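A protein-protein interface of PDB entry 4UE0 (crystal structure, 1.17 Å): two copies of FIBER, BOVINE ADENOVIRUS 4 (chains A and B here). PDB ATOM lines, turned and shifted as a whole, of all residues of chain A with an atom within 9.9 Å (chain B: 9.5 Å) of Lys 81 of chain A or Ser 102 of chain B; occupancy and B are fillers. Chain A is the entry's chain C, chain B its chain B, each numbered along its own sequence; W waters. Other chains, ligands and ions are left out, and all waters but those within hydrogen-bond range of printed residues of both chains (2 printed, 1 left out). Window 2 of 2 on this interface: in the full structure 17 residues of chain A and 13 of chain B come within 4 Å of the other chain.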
ATOM      1  N   THR A  75     -21.361 -18.436   8.665  1.00  0.00           N
ATOM      2  CA  THR A  75     -21.555 -18.969  10.005  1.00  0.00           C
ATOM      3  C   THR A  75     -22.053 -17.895  10.951  1.00  0.00           C
ATOM      4  O   THR A  75     -21.876 -16.695  10.740  1.00  0.00           O
ATOM      5  CB  THR A  75     -20.258 -19.579  10.601  1.00  0.00           C
ATOM      6  OG1 THR A  75     -19.301 -18.552  10.912  1.00  0.00           O
ATOM      7  CG2 THR A  75     -19.658 -20.628   9.704  1.00  0.00           C
ATOM      8  N   GLN A  76     -22.620 -18.379  12.053  1.00  0.00           N
ATOM      9  CA  GLN A  76     -22.819 -17.594  13.276  1.00  0.00           C
ATOM     10  C   GLN A  76     -22.276 -18.404  14.463  1.00  0.00           C
ATOM     11  O   GLN A  76     -22.389 -19.621  14.486  1.00  0.00           O
ATOM     12  CB  GLN A  76     -24.275 -17.265  13.548  1.00  0.00           C
ATOM     13  CG  GLN A  76     -24.884 -16.294  12.560  1.00  0.00           C
ATOM     14  CD  GLN A  76     -26.334 -16.051  12.878  1.00  0.00           C
ATOM     15  OE1 GLN A  76     -27.135 -16.981  12.873  1.00  0.00           O
ATOM     16  NE2 GLN A  76     -26.695 -14.799  13.125  1.00  0.00           N
ATOM     17  N   GLN A  77     -21.752 -17.689  15.460  1.00  0.00           N
ATOM     18  CA  GLN A  77     -21.270 -18.269  16.709  1.00  0.00           C
ATOM     19  C   GLN A  77     -22.317 -18.034  17.801  1.00  0.00           C
ATOM     20  O   GLN A  77     -22.638 -16.888  18.112  1.00  0.00           O
ATOM     21  CB  GLN A  77     -19.927 -17.656  17.082  1.00  0.00           C
ATOM     22  CG  GLN A  77     -19.412 -18.145  18.420  1.00  0.00           C
ATOM     23  CD  GLN A  77     -18.017 -17.681  18.684  1.00  0.00           C
ATOM     24  OE1 GLN A  77     -17.141 -17.737  17.832  1.00  0.00           O
ATOM     25  NE2 GLN A  77     -17.792 -17.212  19.900  1.00  0.00           N
ATOM     26  N   LEU A  78     -22.895 -19.113  18.328  1.00  0.00           N
ATOM     27  CA  LEU A  78     -23.908 -19.016  19.400  1.00  0.00           C
ATOM     28  C   LEU A  78     -23.218 -18.670  20.699  1.00  0.00           C
ATOM     29  O   LEU A  78     -22.023 -18.869  20.841  1.00  0.00           O
ATOM     30  CB  LEU A  78     -24.644 -20.345  19.559  1.00  0.00           C
ATOM     31  CG  LEU A  78     -25.332 -20.869  18.302  1.00  0.00           C
ATOM     32  CD1 LEU A  78     -26.087 -22.158  18.592  1.00  0.00           C
ATOM     33  CD2 LEU A  78     -26.209 -19.799  17.679  1.00  0.00           C
ATOM     34  N   PRO A  79     -23.966 -18.132  21.662  1.00  0.00           N
ATOM     35  CA  PRO A  79     -23.387 -17.773  22.966  1.00  0.00           C
ATOM     36  C   PRO A  79     -22.713 -18.949  23.662  1.00  0.00           C
ATOM     37  O   PRO A  79     -21.706 -18.761  24.352  1.00  0.00           O
ATOM     38  CB  PRO A  79     -24.603 -17.289  23.760  1.00  0.00           C
ATOM     39  CG  PRO A  79     -25.583 -16.841  22.736  1.00  0.00           C
ATOM     40  CD  PRO A  79     -25.386 -17.741  21.557  1.00  0.00           C
ATOM     41  N   ASP A  80     -23.234 -20.158  23.431  1.00  0.00           N
ATOM     42  CA  ASP A  80     -22.631 -21.376  23.989  1.00  0.00           C
ATOM     43  C   ASP A  80     -21.373 -21.807  23.251  1.00  0.00           C
ATOM     44  O   ASP A  80     -20.784 -22.823  23.606  1.00  0.00           O
ATOM     45  CB  ASP A  80     -23.641 -22.548  24.043  1.00  0.00           C
ATOM     46  CG  ASP A  80     -24.245 -22.909  22.680  1.00  0.00           C
ATOM     47  OD1 ASP A  80     -23.558 -22.847  21.654  1.00  0.00           O
ATOM     48  OD2 ASP A  80     -25.441 -23.234  22.643  1.00  0.00           O
ATOM     49  N   LYS A  81     -21.008 -21.059  22.201  1.00  0.00           N
ATOM     50  CA  LYS A  81     -19.796 -21.250  21.391  1.00  0.00           C
ATOM     51  C   LYS A  81     -19.917 -22.294  20.277  1.00  0.00           C
ATOM     52  O   LYS A  81     -18.979 -22.487  19.534  1.00  0.00           O
ATOM     53  CB  LYS A  81     -18.536 -21.572  22.212  1.00  0.00           C
ATOM     54  CG  LYS A  81     -18.235 -20.625  23.355  1.00  0.00           C
ATOM     55  CD  LYS A  81     -17.978 -19.243  22.828  1.00  0.00           C
ATOM     56  CE  LYS A  81     -17.427 -18.350  23.914  1.00  0.00           C
ATOM     57  NZ  LYS A  81     -16.716 -17.199  23.302  1.00  0.00           N
ATOM     58  N   THR A  82     -21.057 -22.959  20.156  1.00  0.00           N
ATOM     59  CA  THR A  82     -21.245 -23.805  18.976  1.00  0.00           C
ATOM     60  C   THR A  82     -21.387 -22.908  17.752  1.00  0.00           C
ATOM     61  O   THR A  82     -21.830 -21.765  17.846  1.00  0.00           O
ATOM     62  CB  THR A  82     -22.454 -24.733  19.078  1.00  0.00           C
ATOM     63  OG1 THR A  82     -23.636 -23.957  19.175  1.00  0.00           O
ATOM     64  CG2 THR A  82     -22.332 -25.612  20.273  1.00  0.00           C
ATOM     65  N   ILE A  83     -20.987 -23.457  16.623  1.00  0.00           N
ATOM     66  CA  ILE A  83     -21.005 -22.736  15.374  1.00  0.00           C
ATOM     67  C   ILE A  83     -22.080 -23.324  14.494  1.00  0.00           C
ATOM     68  O   ILE A  83     -22.141 -24.533  14.266  1.00  0.00           O
ATOM     69  CB  ILE A  83     -19.649 -22.831  14.674  1.00  0.00           C
ATOM     70  CG1 ILE A  83     -18.513 -22.320  15.567  1.00  0.00           C
ATOM     71  CG2 ILE A  83     -19.714 -22.088  13.351  1.00  0.00           C
ATOM     72  CD1 ILE A  83     -18.763 -20.919  16.077  1.00  0.00           C
ATOM     73  N   LYS A  84     -22.935 -22.445  13.979  1.00  0.00           N
ATOM     74  CA  LYS A  84     -23.927 -22.802  12.976  1.00  0.00           C
ATOM     75  C   LYS A  84     -23.445 -22.386  11.590  1.00  0.00           C
ATOM     76  O   LYS A  84     -23.057 -21.235  11.408  1.00  0.00           O
ATOM     77  CB  LYS A  84     -25.248 -22.100  13.267  1.00  0.00           C
ATOM     78  CG  LYS A  84     -25.917 -22.551  14.552  1.00  0.00           C
ATOM     79  CD  LYS A  84     -27.350 -22.067  14.587  1.00  0.00           C
ATOM     80  CE  LYS A  84     -28.231 -23.061  15.328  1.00  0.00           C
ATOM     81  NZ  LYS A  84     -29.517 -22.477  15.807  1.00  0.00           N
ATOM     82  N   ILE A 109     -26.715 -11.756  16.286  1.00  0.00           N
ATOM     83  CA  ILE A 109     -25.426 -12.416  16.279  1.00  0.00           C
ATOM     84  C   ILE A 109     -24.786 -12.160  14.905  1.00  0.00           C
ATOM     85  O   ILE A 109     -25.447 -12.291  13.867  1.00  0.00           O
ATOM     86  CB  ILE A 109     -25.552 -13.925  16.569  1.00  0.00           C
ATOM     87  CG1 ILE A 109     -26.114 -14.152  17.985  1.00  0.00           C
ATOM     88  CG2 ILE A 109     -24.212 -14.626  16.387  1.00  0.00           C
ATOM     89  CD1 ILE A 109     -26.222 -15.609  18.369  1.00  0.00           C
ATOM     90  N   VAL B  49      -4.836 -24.183  21.616  1.00  0.00           N
ATOM     91  CA  VAL B  49      -4.982 -22.738  21.743  1.00  0.00           C
ATOM     92  C   VAL B  49      -6.435 -22.312  21.579  1.00  0.00           C
ATOM     93  O   VAL B  49      -7.128 -22.784  20.677  1.00  0.00           O
ATOM     94  CB  VAL B  49      -4.025 -21.935  20.846  1.00  0.00           C
ATOM     95  CG1 VAL B  49      -2.585 -22.332  21.115  1.00  0.00           C
ATOM     96  CG2 VAL B  49      -4.355 -22.111  19.395  1.00  0.00           C
ATOM     97  N   THR B  50      -6.848 -21.372  22.427  1.00  0.00           N
ATOM     98  CA  THR B  50      -8.130 -20.674  22.263  1.00  0.00           C
ATOM     99  C   THR B  50      -7.932 -19.222  21.815  1.00  0.00           C
ATOM    100  O   THR B  50      -8.790 -18.689  21.115  1.00  0.00           O
ATOM    101  CB  THR B  50      -8.949 -20.703  23.571  1.00  0.00           C
ATOM    102  OG1 THR B  50      -9.133 -22.058  23.971  1.00  0.00           O
ATOM    103  CG2 THR B  50     -10.339 -20.035  23.407  1.00  0.00           C
ATOM    104  N   THR B  51      -6.826 -18.601  22.198  1.00  0.00           N
ATOM    105  CA  THR B  51      -6.584 -17.196  21.873  1.00  0.00           C
ATOM    106  C   THR B  51      -5.153 -17.040  21.381  1.00  0.00           C
ATOM    107  O   THR B  51      -4.211 -17.518  22.028  1.00  0.00           O
ATOM    108  CB  THR B  51      -6.766 -16.289  23.110  1.00  0.00           C
ATOM    109  OG1 THR B  51      -7.982 -16.620  23.773  1.00  0.00           O
ATOM    110  CG2 THR B  51      -6.739 -14.838  22.678  1.00  0.00           C
ATOM    111  N   TYR B  71     -15.420 -10.964  12.580  1.00  0.00           N
ATOM    112  CA  TYR B  71     -15.894 -12.325  12.779  1.00  0.00           C
ATOM    113  C   TYR B  71     -15.746 -13.118  11.503  1.00  0.00           C
ATOM    114  O   TYR B  71     -16.326 -12.756  10.477  1.00  0.00           O
ATOM    115  CB  TYR B  71     -17.367 -12.344  13.296  1.00  0.00           C
ATOM    116  CG  TYR B  71     -17.850 -13.772  13.441  1.00  0.00           C
ATOM    117  CD1 TYR B  71     -17.368 -14.605  14.454  1.00  0.00           C
ATOM    118  CD2 TYR B  71     -18.702 -14.305  12.519  1.00  0.00           C
ATOM    119  CE1 TYR B  71     -17.701 -15.936  14.492  1.00  0.00           C
ATOM    120  CE2 TYR B  71     -19.054 -15.639  12.570  1.00  0.00           C
ATOM    121  CZ  TYR B  71     -18.543 -16.467  13.533  1.00  0.00           C
ATOM    122  OH  TYR B  71     -18.803 -17.832  13.573  1.00  0.00           O
ATOM    123  N   ALA B  72     -15.021 -14.228  11.582  1.00  0.00           N
ATOM    124  CA  ALA B  72     -14.801 -15.109  10.457  1.00  0.00           C
ATOM    125  C   ALA B  72     -14.979 -16.557  10.935  1.00  0.00           C
ATOM    126  O   ALA B  72     -15.276 -16.797  12.108  1.00  0.00           O
ATOM    127  CB  ALA B  72     -13.434 -14.888   9.850  1.00  0.00           C
ATOM    128  N   SER B  73     -14.720 -17.510  10.049  1.00  0.00           N
ATOM    129  CA  SER B  73     -14.710 -18.906  10.444  1.00  0.00           C
ATOM    130  C   SER B  73     -13.565 -19.614   9.800  1.00  0.00           C
ATOM    131  O   SER B  73     -13.025 -19.179   8.771  1.00  0.00           O
ATOM    132  CB  SER B  73     -16.028 -19.572  10.100  1.00  0.00           C
ATOM    133  OG  SER B  73     -16.113 -19.766   8.692  1.00  0.00           O
ATOM    134  N   CYS B  74     -13.186 -20.742  10.399  1.00  0.00           N
ATOM    135  CA  CYS B  74     -12.146 -21.594   9.840  1.00  0.00           C
ATOM    136  C   CYS B  74     -12.433 -23.021  10.265  1.00  0.00           C
ATOM    137  O   CYS B  74     -13.370 -23.262  11.006  1.00  0.00           O
ATOM    138  CB  CYS B  74     -10.773 -21.143  10.299  1.00  0.00           C
ATOM    139  SG  CYS B  74     -10.450 -21.336  12.073  1.00  0.00           S
ATOM    140  N   THR B  75     -11.677 -23.964   9.709  1.00  0.00           N
ATOM    141  CA  THR B  75     -11.906 -25.368  10.004  1.00  0.00           C
ATOM    142  C   THR B  75     -10.596 -26.076  10.267  1.00  0.00           C
ATOM    143  O   THR B  75      -9.517 -25.645   9.867  1.00  0.00           O
ATOM    144  CB  THR B  75     -12.637 -26.096   8.839  1.00  0.00           C
ATOM    145  OG1 THR B  75     -11.786 -26.167   7.694  1.00  0.00           O
ATOM    146  CG2 THR B  75     -13.995 -25.469   8.491  1.00  0.00           C
ATOM    147  N   LYS B  84     -14.268 -29.891  11.914  1.00  0.00           N
ATOM    148  CA  LYS B  84     -14.719 -28.993  12.975  1.00  0.00           C
ATOM    149  C   LYS B  84     -14.575 -27.556  12.479  1.00  0.00           C
ATOM    150  O   LYS B  84     -13.551 -27.192  11.910  1.00  0.00           O
ATOM    151  CB  LYS B  84     -13.927 -29.227  14.256  1.00  0.00           C
ATOM    152  CG  LYS B  84     -14.445 -28.400  15.415  1.00  0.00           C
ATOM    153  CD  LYS B  84     -13.956 -28.919  16.741  1.00  0.00           C
ATOM    154  CE  LYS B  84     -14.545 -28.092  17.869  1.00  0.00           C
ATOM    155  NZ  LYS B  84     -13.919 -28.380  19.190  1.00  0.00           N
ATOM    156  N   THR B  85     -15.646 -26.799  12.683  1.00  0.00           N
ATOM    157  CA  THR B  85     -15.687 -25.397  12.295  1.00  0.00           C
ATOM    158  C   THR B  85     -15.585 -24.545  13.537  1.00  0.00           C
ATOM    159  O   THR B  85     -16.263 -24.795  14.524  1.00  0.00           O
ATOM    160  CB  THR B  85     -16.987 -25.098  11.532  1.00  0.00           C
ATOM    161  OG1 THR B  85     -17.081 -25.969  10.393  1.00  0.00           O
ATOM    162  CG2 THR B  85     -16.994 -23.662  11.023  1.00  0.00           C
ATOM    163  N   TYR B  86     -14.750 -23.518  13.457  1.00  0.00           N
ATOM    164  CA  TYR B  86     -14.515 -22.592  14.559  1.00  0.00           C
ATOM    165  C   TYR B  86     -14.909 -21.176  14.137  1.00  0.00           C
ATOM    166  O   TYR B  86     -14.556 -20.720  13.037  1.00  0.00           O
ATOM    167  CB  TYR B  86     -13.012 -22.546  14.909  1.00  0.00           C
ATOM    168  CG  TYR B  86     -12.413 -23.885  15.225  1.00  0.00           C
ATOM    169  CD1 TYR B  86     -11.899 -24.675  14.233  1.00  0.00           C
ATOM    170  CD2 TYR B  86     -12.377 -24.375  16.521  1.00  0.00           C
ATOM    171  CE1 TYR B  86     -11.381 -25.936  14.512  1.00  0.00           C
ATOM    172  CE2 TYR B  86     -11.830 -25.614  16.812  1.00  0.00           C
ATOM    173  CZ  TYR B  86     -11.318 -26.380  15.803  1.00  0.00           C
ATOM    174  OH  TYR B  86     -10.761 -27.623  16.083  1.00  0.00           O
ATOM    175  N   GLY B  87     -15.559 -20.476  15.052  1.00  0.00           N
ATOM    176  CA  GLY B  87     -15.715 -19.053  14.930  1.00  0.00           C
ATOM    177  C   GLY B  87     -14.438 -18.365  15.318  1.00  0.00           C
ATOM    178  O   GLY B  87     -13.757 -18.779  16.264  1.00  0.00           O
ATOM    179  N   VAL B  88     -14.111 -17.292  14.604  1.00  0.00           N
ATOM    180  CA  VAL B  88     -12.895 -16.535  14.834  1.00  0.00           C
ATOM    181  C   VAL B  88     -13.294 -15.080  15.076  1.00  0.00           C
ATOM    182  O   VAL B  88     -13.849 -14.447  14.179  1.00  0.00           O
ATOM    183  CB  VAL B  88     -11.913 -16.611  13.660  1.00  0.00           C
ATOM    184  CG1 VAL B  88     -10.589 -15.970  14.009  1.00  0.00           C
ATOM    185  CG2 VAL B  88     -11.692 -18.040  13.189  1.00  0.00           C
ATOM    186  N   THR B  89     -13.021 -14.563  16.272  1.00  0.00           N
ATOM    187  CA  THR B  89     -13.400 -13.185  16.624  1.00  0.00           C
ATOM    188  C   THR B  89     -12.110 -12.427  16.872  1.00  0.00           C
ATOM    189  O   THR B  89     -11.301 -12.834  17.718  1.00  0.00           O
ATOM    190  CB  THR B  89     -14.286 -13.169  17.874  1.00  0.00           C
ATOM    191  OG1 THR B  89     -15.477 -13.913  17.608  1.00  0.00           O
ATOM    192  CG2 THR B  89     -14.671 -11.749  18.235  1.00  0.00           C
ATOM    193  N   ILE B  90     -11.905 -11.350  16.125  1.00  0.00           N
ATOM    194  CA  ILE B  90     -10.653 -10.596  16.195  1.00  0.00           C
ATOM    195  C   ILE B  90     -10.952  -9.178  16.676  1.00  0.00           C
ATOM    196  O   ILE B  90     -11.738  -8.446  16.066  1.00  0.00           O
ATOM    197  CB  ILE B  90      -9.852 -10.562  14.876  1.00  0.00           C
ATOM    198  CG1 ILE B  90      -9.771 -11.955  14.231  1.00  0.00           C
ATOM    199  CG2 ILE B  90      -8.482  -9.998  15.159  1.00  0.00           C
ATOM    200  CD1 ILE B  90     -10.855 -12.233  13.204  1.00  0.00           C
ATOM    201  N   ILE B  99      -7.092 -12.812  18.764  1.00  0.00           N
ATOM    202  CA  ILE B  99      -7.792 -13.711  17.837  1.00  0.00           C
ATOM    203  C   ILE B  99      -8.349 -14.850  18.684  1.00  0.00           C
ATOM    204  O   ILE B  99      -7.576 -15.668  19.216  1.00  0.00           O
ATOM    205  CB  ILE B  99      -6.845 -14.259  16.761  1.00  0.00           C
ATOM    206  CG1 ILE B  99      -6.180 -13.147  15.963  1.00  0.00           C
ATOM    207  CG2 ILE B  99      -7.580 -15.234  15.859  1.00  0.00           C
ATOM    208  CD1 ILE B  99      -5.036 -13.623  15.122  1.00  0.00           C
ATOM    209  N   ASN B 100      -9.671 -14.855  18.888  1.00  0.00           N
ATOM    210  CA  ASN B 100     -10.337 -15.810  19.764  1.00  0.00           C
ATOM    211  C   ASN B 100     -11.067 -16.839  18.919  1.00  0.00           C
ATOM    212  O   ASN B 100     -11.915 -16.496  18.107  1.00  0.00           O
ATOM    213  CB  ASN B 100     -11.292 -15.090  20.730  1.00  0.00           C
ATOM    214  CG  ASN B 100     -10.579 -14.631  21.961  1.00  0.00           C
ATOM    215  OD1 ASN B 100     -10.195 -15.457  22.776  1.00  0.00           O
ATOM    216  ND2 ASN B 100     -10.347 -13.362  22.084  1.00  0.00           N
ATOM    217  N   PHE B 101     -10.761 -18.101  19.189  1.00  0.00           N
ATOM    218  CA  PHE B 101     -11.428 -19.207  18.527  1.00  0.00           C
ATOM    219  C   PHE B 101     -12.563 -19.661  19.432  1.00  0.00           C
ATOM    220  O   PHE B 101     -12.421 -19.680  20.657  1.00  0.00           O
ATOM    221  CB  PHE B 101     -10.434 -20.339  18.237  1.00  0.00           C
ATOM    222  CG  PHE B 101      -9.335 -19.925  17.308  1.00  0.00           C
ATOM    223  CD1 PHE B 101      -9.539 -19.961  15.932  1.00  0.00           C
ATOM    224  CD2 PHE B 101      -8.161 -19.360  17.782  1.00  0.00           C
ATOM    225  CE1 PHE B 101      -8.573 -19.502  15.059  1.00  0.00           C
ATOM    226  CE2 PHE B 101      -7.194 -18.902  16.917  1.00  0.00           C
ATOM    227  CZ  PHE B 101      -7.401 -18.973  15.546  1.00  0.00           C
ATOM    228  N   SER B 102     -13.657 -20.103  18.839  1.00  0.00           N
ATOM    229  CA  SER B 102     -14.853 -20.459  19.600  1.00  0.00           C
ATOM    230  C   SER B 102     -14.648 -21.652  20.532  1.00  0.00           C
ATOM    231  O   SER B 102     -15.329 -21.764  21.563  1.00  0.00           O
ATOM    232  CB  SER B 102     -15.994 -20.743  18.642  1.00  0.00           C
ATOM    233  OG  SER B 102     -15.618 -21.699  17.670  1.00  0.00           O
ATOM    234  N   SER B 103     -13.718 -22.529  20.151  1.00  0.00           N
ATOM    235  CA  SER B 103     -13.317 -23.625  21.016  1.00  0.00           C
ATOM    236  C   SER B 103     -11.833 -23.823  20.781  1.00  0.00           C
ATOM    237  O   SER B 103     -11.290 -23.353  19.794  1.00  0.00           O
ATOM    238  CB  SER B 103     -14.211 -24.870  20.783  1.00  0.00           C
ATOM    239  OG  SER B 103     -13.973 -25.460  19.572  1.00  0.00           O
ATOM    240  N   SER B 104     -11.166 -24.511  21.693  1.00  0.00           N
ATOM    241  CA  SER B 104      -9.746 -24.718  21.556  1.00  0.00           C
ATOM    242  C   SER B 104      -9.436 -25.556  20.292  1.00  0.00           C
ATOM    243  O   SER B 104     -10.153 -26.520  19.977  1.00  0.00           O
ATOM    244  CB  SER B 104      -9.172 -25.415  22.799  1.00  0.00           C
ATOM    245  OG  SER B 104      -9.800 -26.657  23.025  1.00  0.00           O
ATOM    246  N   LEU B 105      -8.354 -25.195  19.615  1.00  0.00           N
ATOM    247  CA  LEU B 105      -7.967 -25.865  18.414  1.00  0.00           C
ATOM    248  C   LEU B 105      -7.358 -27.214  18.769  1.00  0.00           C
ATOM    249  O   LEU B 105      -6.844 -27.427  19.865  1.00  0.00           O
ATOM    250  CB  LEU B 105      -6.967 -24.995  17.655  1.00  0.00           C
ATOM    251  CG  LEU B 105      -7.492 -23.630  17.178  1.00  0.00           C
ATOM    252  CD1 LEU B 105      -6.348 -22.799  16.604  1.00  0.00           C
ATOM    253  CD2 LEU B 105      -8.573 -23.803  16.128  1.00  0.00           C
HETATM  254  O   HOH W   1     -16.604 -23.990  18.635  1.00  0.00           O
HETATM  255  O   HOH W   2     -13.678 -18.409  22.641  1.00  0.00           O
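OH of Tyr 71 of chain B sits at hydrogen-bond distance from OG1 of Thr 75 of chain A (2.8 Å).
The backbone NH of Gly 87 of chain B sits at hydrogen-bond distance from the side-chain hydroxyl of Ser 102 of chain B (2.9 Å).
O of Gln 76 of chain A lies within hydrogen-bond range of N of Lys 84 of chain A, 2.9 Å away.
The backbone carbonyl oxygen (O) of Ile 109 of chain A is in hydrogen-bond range of the side-chain amide nitrogen (NE2) of Gln 76 of chain A (2.9 Å).
Thr 75 of chain A touches Ser 73 of chain B (OG1 to CB, 3.5 Å).
Tyr 71 of chain B touches Gln 76 of chain A (OH to C, 3.6 Å).
Gln 77 of chain A touches Tyr 71 of chain B (N to OH, 3.5 Å).
OE1 of Gln 77 of chain A touches CA of Gly 87 of chain B, at 3.5 Å.
Gln 77 of chain A touches Ser 102 of chain B (OE1 to CB, 3.3 Å).
Lys 81 of chain A touches Ser 102 of chain B (CB to O, 3.3 Å).
Tyr 71 of chain B touches Ile 83 of chain A.
Ile 83 of chain A touches Thr 85 of chain B (CG1 to O, 3.5 Å).
Ile 83 of chain A touches Gly 87 of chain B (CD1 to N, 3.4 Å).
OG of Ser 102 of chain B touches CD1 of Ile 83 of chain A, 3.6 Å away.
Of the printed residues of chain B, Gln 76 of chain A touches Tyr 71.
Leu 78 of chain A touches none of the printed residues of chain B.
Asp 80 of chain A touches none of the printed residues of chain B.
Lys 81 of chain A touches just one residue of chain B: Ser 102.
No residue of chain B comes within 4 Å of Thr 82 of chain A.
Of the printed residues of chain B, Ile 83 of chain A touches Tyr 71 (3.98 Å), Thr 85 (3.5 Å), Gly 87 (3.4 Å) and Ser 102 (3.6 Å).
Printed residues of chain A within 4 Å of Gly 87 of chain B: Gln 77 and Ile 83.
Ser 102 of chain B touches three residues of chain A.
No residue of chain A comes within 4 Å of Ser 103 of chain B.
The nearest residue of chain B that does not touch Lys 81 of chain A is Ser 103 of chain B (5.3 Å).
Of the 22 printed residues of chain B, 5 touch a printed residue of chain A.
Hydrophobic or aromatic side chains of chain A within 4 Å of the printed part of chain B: Ile 83.
Among the printed residues, 11 pairs touch across the chains.
2 positions are printed for both chains.
Water W2 bridges the backbone carbonyl oxygen (O) of Phe 101 of chain B (2.7 Å) and the side-chain amino group (NZ) of Lys 81 of chain A (3.3 Å).
Water W1 lies within hydrogen-bond range of OG of Ser 102 of chain B (2.7 Å), O of Lys 81 of chain A (3.0 Å) and OG of Ser 103 of chain B (3.2 Å).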
